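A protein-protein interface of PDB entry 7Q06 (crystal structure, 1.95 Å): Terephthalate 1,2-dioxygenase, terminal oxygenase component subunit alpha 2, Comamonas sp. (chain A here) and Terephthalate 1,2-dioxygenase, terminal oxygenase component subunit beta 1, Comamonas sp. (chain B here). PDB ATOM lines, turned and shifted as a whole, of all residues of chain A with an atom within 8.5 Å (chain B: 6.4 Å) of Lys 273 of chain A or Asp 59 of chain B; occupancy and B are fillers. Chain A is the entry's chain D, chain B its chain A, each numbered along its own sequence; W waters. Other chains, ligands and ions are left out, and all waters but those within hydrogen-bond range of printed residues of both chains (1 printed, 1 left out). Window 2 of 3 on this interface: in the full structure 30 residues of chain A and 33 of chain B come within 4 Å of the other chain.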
ATOM      1  N   PHE A 223     -12.082  19.251 -33.586  1.00  0.00           N
ATOM      2  CA  PHE A 223     -11.329  20.545 -33.497  1.00  0.00           C
ATOM      3  C   PHE A 223     -11.577  21.402 -34.769  1.00  0.00           C
ATOM      4  O   PHE A 223     -10.778  22.297 -35.081  1.00  0.00           O
ATOM      5  CB  PHE A 223      -9.867  20.264 -33.087  1.00  0.00           C
ATOM      6  CG  PHE A 223      -9.750  19.529 -31.761  1.00  0.00           C
ATOM      7  CD1 PHE A 223     -10.278  20.079 -30.592  1.00  0.00           C
ATOM      8  CD2 PHE A 223      -9.195  18.245 -31.685  1.00  0.00           C
ATOM      9  CE1 PHE A 223     -10.230  19.384 -29.391  1.00  0.00           C
ATOM     10  CE2 PHE A 223      -9.142  17.555 -30.479  1.00  0.00           C
ATOM     11  CZ  PHE A 223      -9.653  18.129 -29.334  1.00  0.00           C
ATOM     12  N   TYR A 270     -13.902  15.502 -25.437  1.00  0.00           N
ATOM     13  CA  TYR A 270     -12.453  15.435 -25.770  1.00  0.00           C
ATOM     14  C   TYR A 270     -11.847  16.865 -25.827  1.00  0.00           C
ATOM     15  O   TYR A 270     -12.317  17.640 -26.706  1.00  0.00           O
ATOM     16  CB  TYR A 270     -12.263  14.605 -27.056  1.00  0.00           C
ATOM     17  CG  TYR A 270     -10.810  14.296 -27.322  1.00  0.00           C
ATOM     18  CD1 TYR A 270     -10.181  13.219 -26.718  1.00  0.00           C
ATOM     19  CD2 TYR A 270     -10.028  15.175 -28.060  1.00  0.00           C
ATOM     20  CE1 TYR A 270      -8.821  13.004 -26.878  1.00  0.00           C
ATOM     21  CE2 TYR A 270      -8.665  14.982 -28.220  1.00  0.00           C
ATOM     22  CZ  TYR A 270      -8.058  13.886 -27.630  1.00  0.00           C
ATOM     23  OH  TYR A 270      -6.712  13.676 -27.790  1.00  0.00           O
ATOM     24  N   ARG A 271     -10.827  17.160 -24.973  1.00  0.00           N
ATOM     25  CA  ARG A 271     -10.045  18.446 -24.835  1.00  0.00           C
ATOM     26  C   ARG A 271      -8.505  18.224 -24.813  1.00  0.00           C
ATOM     27  O   ARG A 271      -8.106  17.056 -24.841  1.00  0.00           O
ATOM     28  CB  ARG A 271     -10.516  19.161 -23.563  1.00  0.00           C
ATOM     29  CG  ARG A 271     -11.713  20.081 -23.770  1.00  0.00           C
ATOM     30  CD  ARG A 271     -11.448  21.192 -24.791  1.00  0.00           C
ATOM     31  NE  ARG A 271     -10.144  21.867 -24.653  1.00  0.00           N
ATOM     32  CZ  ARG A 271      -9.203  21.991 -25.608  1.00  0.00           C
ATOM     33  NH1 ARG A 271      -9.381  21.456 -26.808  1.00  0.00           N
ATOM     34  NH2 ARG A 271      -8.071  22.636 -25.345  1.00  0.00           N
ATOM     35  N   LEU A 272      -7.671  19.301 -24.762  1.00  0.00           N
ATOM     36  CA  LEU A 272      -6.168  19.289 -24.857  1.00  0.00           C
ATOM     37  C   LEU A 272      -5.576  20.123 -23.716  1.00  0.00           C
ATOM     38  O   LEU A 272      -5.871  21.345 -23.714  1.00  0.00           O
ATOM     39  CB  LEU A 272      -5.623  19.926 -26.153  1.00  0.00           C
ATOM     40  CG  LEU A 272      -5.972  19.267 -27.490  1.00  0.00           C
ATOM     41  CD1 LEU A 272      -5.335  20.043 -28.635  1.00  0.00           C
ATOM     42  CD2 LEU A 272      -5.534  17.806 -27.548  1.00  0.00           C
ATOM     43  N   LYS A 273      -4.698  19.545 -22.875  1.00  0.00           N
ATOM     44  CA  LYS A 273      -3.960  20.315 -21.832  1.00  0.00           C
ATOM     45  C   LYS A 273      -2.931  21.237 -22.489  1.00  0.00           C
ATOM     46  O   LYS A 273      -2.455  22.167 -21.825  1.00  0.00           O
ATOM     47  CB  LYS A 273      -3.134  19.438 -20.881  1.00  0.00           C
ATOM     48  CG  LYS A 273      -3.856  18.457 -19.979  1.00  0.00           C
ATOM     49  CD  LYS A 273      -2.967  18.079 -18.810  1.00  0.00           C
ATOM     50  CE  LYS A 273      -3.537  16.956 -17.983  1.00  0.00           C
ATOM     51  NZ  LYS A 273      -4.944  17.243 -17.625  1.00  0.00           N
ATOM     52  N   ASP A 274      -2.481  20.924 -23.702  1.00  0.00           N
ATOM     53  CA  ASP A 274      -1.485  21.756 -24.413  1.00  0.00           C
ATOM     54  C   ASP A 274      -2.062  22.056 -25.782  1.00  0.00           C
ATOM     55  O   ASP A 274      -1.866  21.303 -26.739  1.00  0.00           O
ATOM     56  CB  ASP A 274      -0.116  21.085 -24.436  1.00  0.00           C
ATOM     57  CG  ASP A 274       0.977  22.043 -24.846  1.00  0.00           C
ATOM     58  OD1 ASP A 274       0.681  22.960 -25.659  1.00  0.00           O
ATOM     59  OD2 ASP A 274       2.108  21.842 -24.374  1.00  0.00           O
ATOM     60  N   PRO A 275      -2.860  23.145 -25.881  1.00  0.00           N
ATOM     61  CA  PRO A 275      -3.428  23.548 -27.164  1.00  0.00           C
ATOM     62  C   PRO A 275      -2.353  23.978 -28.178  1.00  0.00           C
ATOM     63  O   PRO A 275      -2.719  24.178 -29.307  1.00  0.00           O
ATOM     64  CB  PRO A 275      -4.345  24.741 -26.829  1.00  0.00           C
ATOM     65  CG  PRO A 275      -4.511  24.701 -25.316  1.00  0.00           C
ATOM     66  CD  PRO A 275      -3.269  24.014 -24.769  1.00  0.00           C
ATOM     67  N   SER A 276      -1.082  24.146 -27.779  1.00  0.00           N
ATOM     68  CA  SER A 276       0.008  24.553 -28.718  1.00  0.00           C
ATOM     69  C   SER A 276       0.122  23.542 -29.881  1.00  0.00           C
ATOM     70  O   SER A 276       0.601  23.927 -30.945  1.00  0.00           O
ATOM     71  CB  SER A 276       1.341  24.776 -28.034  1.00  0.00           C
ATOM     72  OG  SER A 276       1.912  23.572 -27.540  1.00  0.00           O
ATOM     73  N   LEU A 277      -0.322  22.288 -29.703  1.00  0.00           N
ATOM     74  CA  LEU A 277      -0.401  21.287 -30.801  1.00  0.00           C
ATOM     75  C   LEU A 277      -1.013  21.919 -32.059  1.00  0.00           C
ATOM     76  O   LEU A 277      -0.517  21.610 -33.137  1.00  0.00           O
ATOM     77  CB  LEU A 277      -1.235  20.085 -30.357  1.00  0.00           C
ATOM     78  CG  LEU A 277      -1.562  19.086 -31.474  1.00  0.00           C
ATOM     79  CD1 LEU A 277      -0.277  18.542 -32.108  1.00  0.00           C
ATOM     80  CD2 LEU A 277      -2.416  17.951 -30.921  1.00  0.00           C
ATOM     81  N   PHE A 353      -2.113  12.042 -35.431  1.00  0.00           N
ATOM     82  CA  PHE A 353      -3.490  12.138 -34.911  1.00  0.00           C
ATOM     83  C   PHE A 353      -4.518  12.034 -36.077  1.00  0.00           C
ATOM     84  O   PHE A 353      -5.635  11.595 -35.836  1.00  0.00           O
ATOM     85  CB  PHE A 353      -3.610  13.412 -34.072  1.00  0.00           C
ATOM     86  CG  PHE A 353      -2.734  13.431 -32.838  1.00  0.00           C
ATOM     87  CD1 PHE A 353      -2.674  12.345 -31.988  1.00  0.00           C
ATOM     88  CD2 PHE A 353      -1.980  14.546 -32.517  1.00  0.00           C
ATOM     89  CE1 PHE A 353      -1.878  12.387 -30.834  1.00  0.00           C
ATOM     90  CE2 PHE A 353      -1.207  14.605 -31.360  1.00  0.00           C
ATOM     91  CZ  PHE A 353      -1.157  13.524 -30.520  1.00  0.00           C
ATOM     92  N   PRO B  27       3.363   9.765 -18.853  1.00  0.00           N
ATOM     93  CA  PRO B  27       3.846  11.130 -18.696  1.00  0.00           C
ATOM     94  C   PRO B  27       4.555  11.386 -17.367  1.00  0.00           C
ATOM     95  O   PRO B  27       5.427  12.238 -17.343  1.00  0.00           O
ATOM     96  CB  PRO B  27       2.557  11.978 -18.785  1.00  0.00           C
ATOM     97  CG  PRO B  27       1.662  11.153 -19.668  1.00  0.00           C
ATOM     98  CD  PRO B  27       1.935   9.732 -19.194  1.00  0.00           C
ATOM     99  N   LYS B  32       8.342  18.331 -16.294  1.00  0.00           N
ATOM    100  CA  LYS B  32       7.300  19.250 -16.811  1.00  0.00           C
ATOM    101  C   LYS B  32       7.669  19.803 -18.190  1.00  0.00           C
ATOM    102  O   LYS B  32       6.779  19.875 -19.042  1.00  0.00           O
ATOM    103  CB  LYS B  32       7.116  20.422 -15.828  1.00  0.00           C
ATOM    104  CG  LYS B  32       5.667  20.830 -15.604  1.00  0.00           C
ATOM    105  CD  LYS B  32       4.786  19.721 -14.987  1.00  0.00           C
ATOM    106  CE  LYS B  32       3.303  19.928 -15.264  1.00  0.00           C
ATOM    107  NZ  LYS B  32       2.921  21.346 -15.067  1.00  0.00           N
ATOM    108  N   CYS B  34       9.841  18.580 -20.523  1.00  0.00           N
ATOM    109  CA  CYS B  34      10.683  17.499 -21.107  1.00  0.00           C
ATOM    110  C   CYS B  34      10.723  17.609 -22.622  1.00  0.00           C
ATOM    111  O   CYS B  34       9.908  18.369 -23.212  1.00  0.00           O
ATOM    112  CB  CYS B  34      10.082  16.152 -20.763  1.00  0.00           C
ATOM    113  SG  CYS B  34       8.385  15.994 -21.361  1.00  0.00           S
ATOM    114  N   SER B  57       6.593  19.215 -23.857  1.00  0.00           N
ATOM    115  CA  SER B  57       6.021  19.368 -22.509  1.00  0.00           C
ATOM    116  C   SER B  57       5.427  18.044 -22.046  1.00  0.00           C
ATOM    117  O   SER B  57       5.013  17.230 -22.916  1.00  0.00           O
ATOM    118  CB  SER B  57       4.991  20.458 -22.528  1.00  0.00           C
ATOM    119  OG  SER B  57       3.770  19.963 -23.057  1.00  0.00           O
ATOM    120  N   GLN B  58       5.279  17.872 -20.734  1.00  0.00           N
ATOM    121  CA  GLN B  58       4.616  16.675 -20.187  1.00  0.00           C
ATOM    122  C   GLN B  58       3.147  16.665 -20.650  1.00  0.00           C
ATOM    123  O   GLN B  58       2.535  15.573 -20.902  1.00  0.00           O
ATOM    124  CB  GLN B  58       4.821  16.661 -18.669  1.00  0.00           C
ATOM    125  CG  GLN B  58       4.258  15.399 -18.028  1.00  0.00           C
ATOM    126  CD  GLN B  58       4.171  15.547 -16.537  1.00  0.00           C
ATOM    127  OE1 GLN B  58       3.263  16.189 -16.029  1.00  0.00           O
ATOM    128  NE2 GLN B  58       5.090  14.922 -15.821  1.00  0.00           N
ATOM    129  N   ASP B  59       2.545  17.829 -20.744  1.00  0.00           N
ATOM    130  CA  ASP B  59       1.112  17.939 -21.164  1.00  0.00           C
ATOM    131  C   ASP B  59       0.908  17.450 -22.619  1.00  0.00           C
ATOM    132  O   ASP B  59      -0.153  16.843 -22.901  1.00  0.00           O
ATOM    133  CB  ASP B  59       0.626  19.374 -20.996  1.00  0.00           C
ATOM    134  CG  ASP B  59       0.615  19.784 -19.538  1.00  0.00           C
ATOM    135  OD1 ASP B  59       0.130  18.943 -18.716  1.00  0.00           O
ATOM    136  OD2 ASP B  59       1.190  20.836 -19.250  1.00  0.00           O
ATOM    137  N   MET B  60       1.880  17.641 -23.506  1.00  0.00           N
ATOM    138  CA  MET B  60       1.784  17.037 -24.868  1.00  0.00           C
ATOM    139  C   MET B  60       1.771  15.511 -24.753  1.00  0.00           C
ATOM    140  O   MET B  60       1.008  14.861 -25.493  1.00  0.00           O
ATOM    141  CB  MET B  60       2.907  17.502 -25.783  1.00  0.00           C
ATOM    142  CG  MET B  60       2.667  18.898 -26.322  1.00  0.00           C
ATOM    143  SD  MET B  60       3.890  19.379 -27.567  1.00  0.00           S
ATOM    144  CE  MET B  60       3.243  18.427 -28.934  1.00  0.00           C
ATOM    145  N   LEU B  61       2.488  14.940 -23.777  1.00  0.00           N
ATOM    146  CA  LEU B  61       2.490  13.477 -23.571  1.00  0.00           C
ATOM    147  C   LEU B  61       1.084  13.049 -23.128  1.00  0.00           C
ATOM    148  O   LEU B  61       0.550  12.050 -23.659  1.00  0.00           O
ATOM    149  CB  LEU B  61       3.573  13.071 -22.556  1.00  0.00           C
ATOM    150  CG  LEU B  61       5.008  13.532 -22.885  1.00  0.00           C
ATOM    151  CD1 LEU B  61       6.006  12.934 -21.889  1.00  0.00           C
ATOM    152  CD2 LEU B  61       5.440  13.155 -24.291  1.00  0.00           C
ATOM    153  N   THR B  62       0.487  13.772 -22.188  1.00  0.00           N
ATOM    154  CA  THR B  62      -0.867  13.474 -21.645  1.00  0.00           C
ATOM    155  C   THR B  62      -1.885  13.543 -22.796  1.00  0.00           C
ATOM    156  O   THR B  62      -2.733  12.633 -22.924  1.00  0.00           O
ATOM    157  CB  THR B  62      -1.193  14.433 -20.489  1.00  0.00           C
ATOM    158  OG1 THR B  62      -0.120  14.281 -19.565  1.00  0.00           O
ATOM    159  CG2 THR B  62      -2.527  14.154 -19.824  1.00  0.00           C
ATOM    160  N   ASP B  63      -1.797  14.570 -23.621  1.00  0.00           N
ATOM    161  CA  ASP B  63      -2.702  14.709 -24.799  1.00  0.00           C
ATOM    162  C   ASP B  63      -2.585  13.508 -25.721  1.00  0.00           C
ATOM    163  O   ASP B  63      -3.631  13.026 -26.242  1.00  0.00           O
ATOM    164  CB  ASP B  63      -2.397  15.979 -25.569  1.00  0.00           C
ATOM    165  CG  ASP B  63      -2.884  17.201 -24.816  1.00  0.00           C
ATOM    166  OD1 ASP B  63      -3.774  17.014 -23.965  1.00  0.00           O
ATOM    167  OD2 ASP B  63      -2.359  18.312 -25.065  1.00  0.00           O
ATOM    168  N   ARG B  64      -1.373  12.984 -25.880  1.00  0.00           N
ATOM    169  CA  ARG B  64      -1.193  11.874 -26.831  1.00  0.00           C
ATOM    170  C   ARG B  64      -1.901  10.654 -26.260  1.00  0.00           C
ATOM    171  O   ARG B  64      -2.547   9.858 -27.054  1.00  0.00           O
ATOM    172  CB  ARG B  64       0.279  11.671 -27.206  1.00  0.00           C
ATOM    173  CG  ARG B  64       0.409  10.619 -28.293  1.00  0.00           C
ATOM    174  CD  ARG B  64       1.726  10.675 -28.987  1.00  0.00           C
ATOM    175  NE  ARG B  64       1.770  11.583 -30.117  1.00  0.00           N
ATOM    176  CZ  ARG B  64       1.426  11.258 -31.353  1.00  0.00           C
ATOM    177  NH1 ARG B  64       0.843  10.097 -31.642  1.00  0.00           N
ATOM    178  NH2 ARG B  64       1.607  12.137 -32.333  1.00  0.00           N
HETATM  179  O   HOH W   1      -0.827  18.584 -27.148  1.00  0.00           O
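The backbone NH (N) of Lys 273 of chain A is in hydrogen-bond range of the side-chain carboxylate (OD1) of Asp 63 of chain B (2.9 Å).
OD2 of Asp 274 of chain A lies within hydrogen-bond range of OG of Ser 57 of chain B.
The backbone NH (N) of Asp 274 of chain A is in hydrogen-bond range of the side-chain carboxylate (OD2) of Asp 63 of chain B.
O of Cys 34 of chain B sits at hydrogen-bond distance from N of Ser 57 of chain B (3.5 Å).
OG of Ser 57 of chain B sits close to N of Asp 59 of chain B, 3.4 Å away.
The backbone carbonyl oxygen (O) of Gln 58 of chain B lies within hydrogen-bond range of the side-chain hydroxyl (OG1) of Thr 62 of chain B.
N of Met 60 of chain B lies within hydrogen-bond range of OG of Ser 57 of chain B (3.0 Å).
N of Ser 276 of chain A sits at hydrogen-bond distance from OD1 of Asp 274 of chain A (3.0 Å).
Among the printed residues, pairs that only touch across the chains: Lys 273 of chain A with Asp 59 of chain B (3.2 Å), Leu 272 of chain A with Asp 63 of chain B (3.4 Å), Lys 273 of chain A with Thr 62 of chain B (3.5 Å), Tyr 270 of chain A with Asp 63 of chain B (3.5 Å), Phe 353 of chain A with Arg 64 of chain B (3.5 Å), Asp 274 of chain A with Met 60 of chain B (3.6 Å) and Asp 274 of chain A with Asp 59 of chain B (3.9 Å).
Of the printed residues of chain B, Lys 273 of chain A touches Asp 59 (3.2 Å), Thr 62 (3.5 Å) and Asp 63 (2.9 Å).
Asp 59 of chain B touches just these residues of chain A: Lys 273 and Asp 274.
Of the printed residues of chain A, Met 60 of chain B touches Asp 274.
Of the printed residues of chain B, Leu 272 of chain A touches Asp 63 (3.4 Å).
Of the printed residues of chain A, Thr 62 of chain B touches Lys 273 (3.5 Å).
Cys 34 of chain B touches none of the printed residues of chain A.
Of the 11 printed residues of chain B, 6 touch a printed residue of chain A.
Along chain B the printed residues that touch a printed residue of chain A span positions 57 to 64.
Hydrophobic or aromatic side chains of chain A within 4 Å of the printed part of chain B: Tyr 270, Leu 272 and Phe 353.
Among the printed residues, no Asp or Glu carboxylate lies within 4 Å of a Lys or Arg side-chain nitrogen of the other chain.
Water W1 lies within hydrogen-bond range of the side-chain carboxylate of Asp 63 of chain B (2.6 Å) and the backbone carbonyl oxygen of Asp 274 of chain A (2.9 Å).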
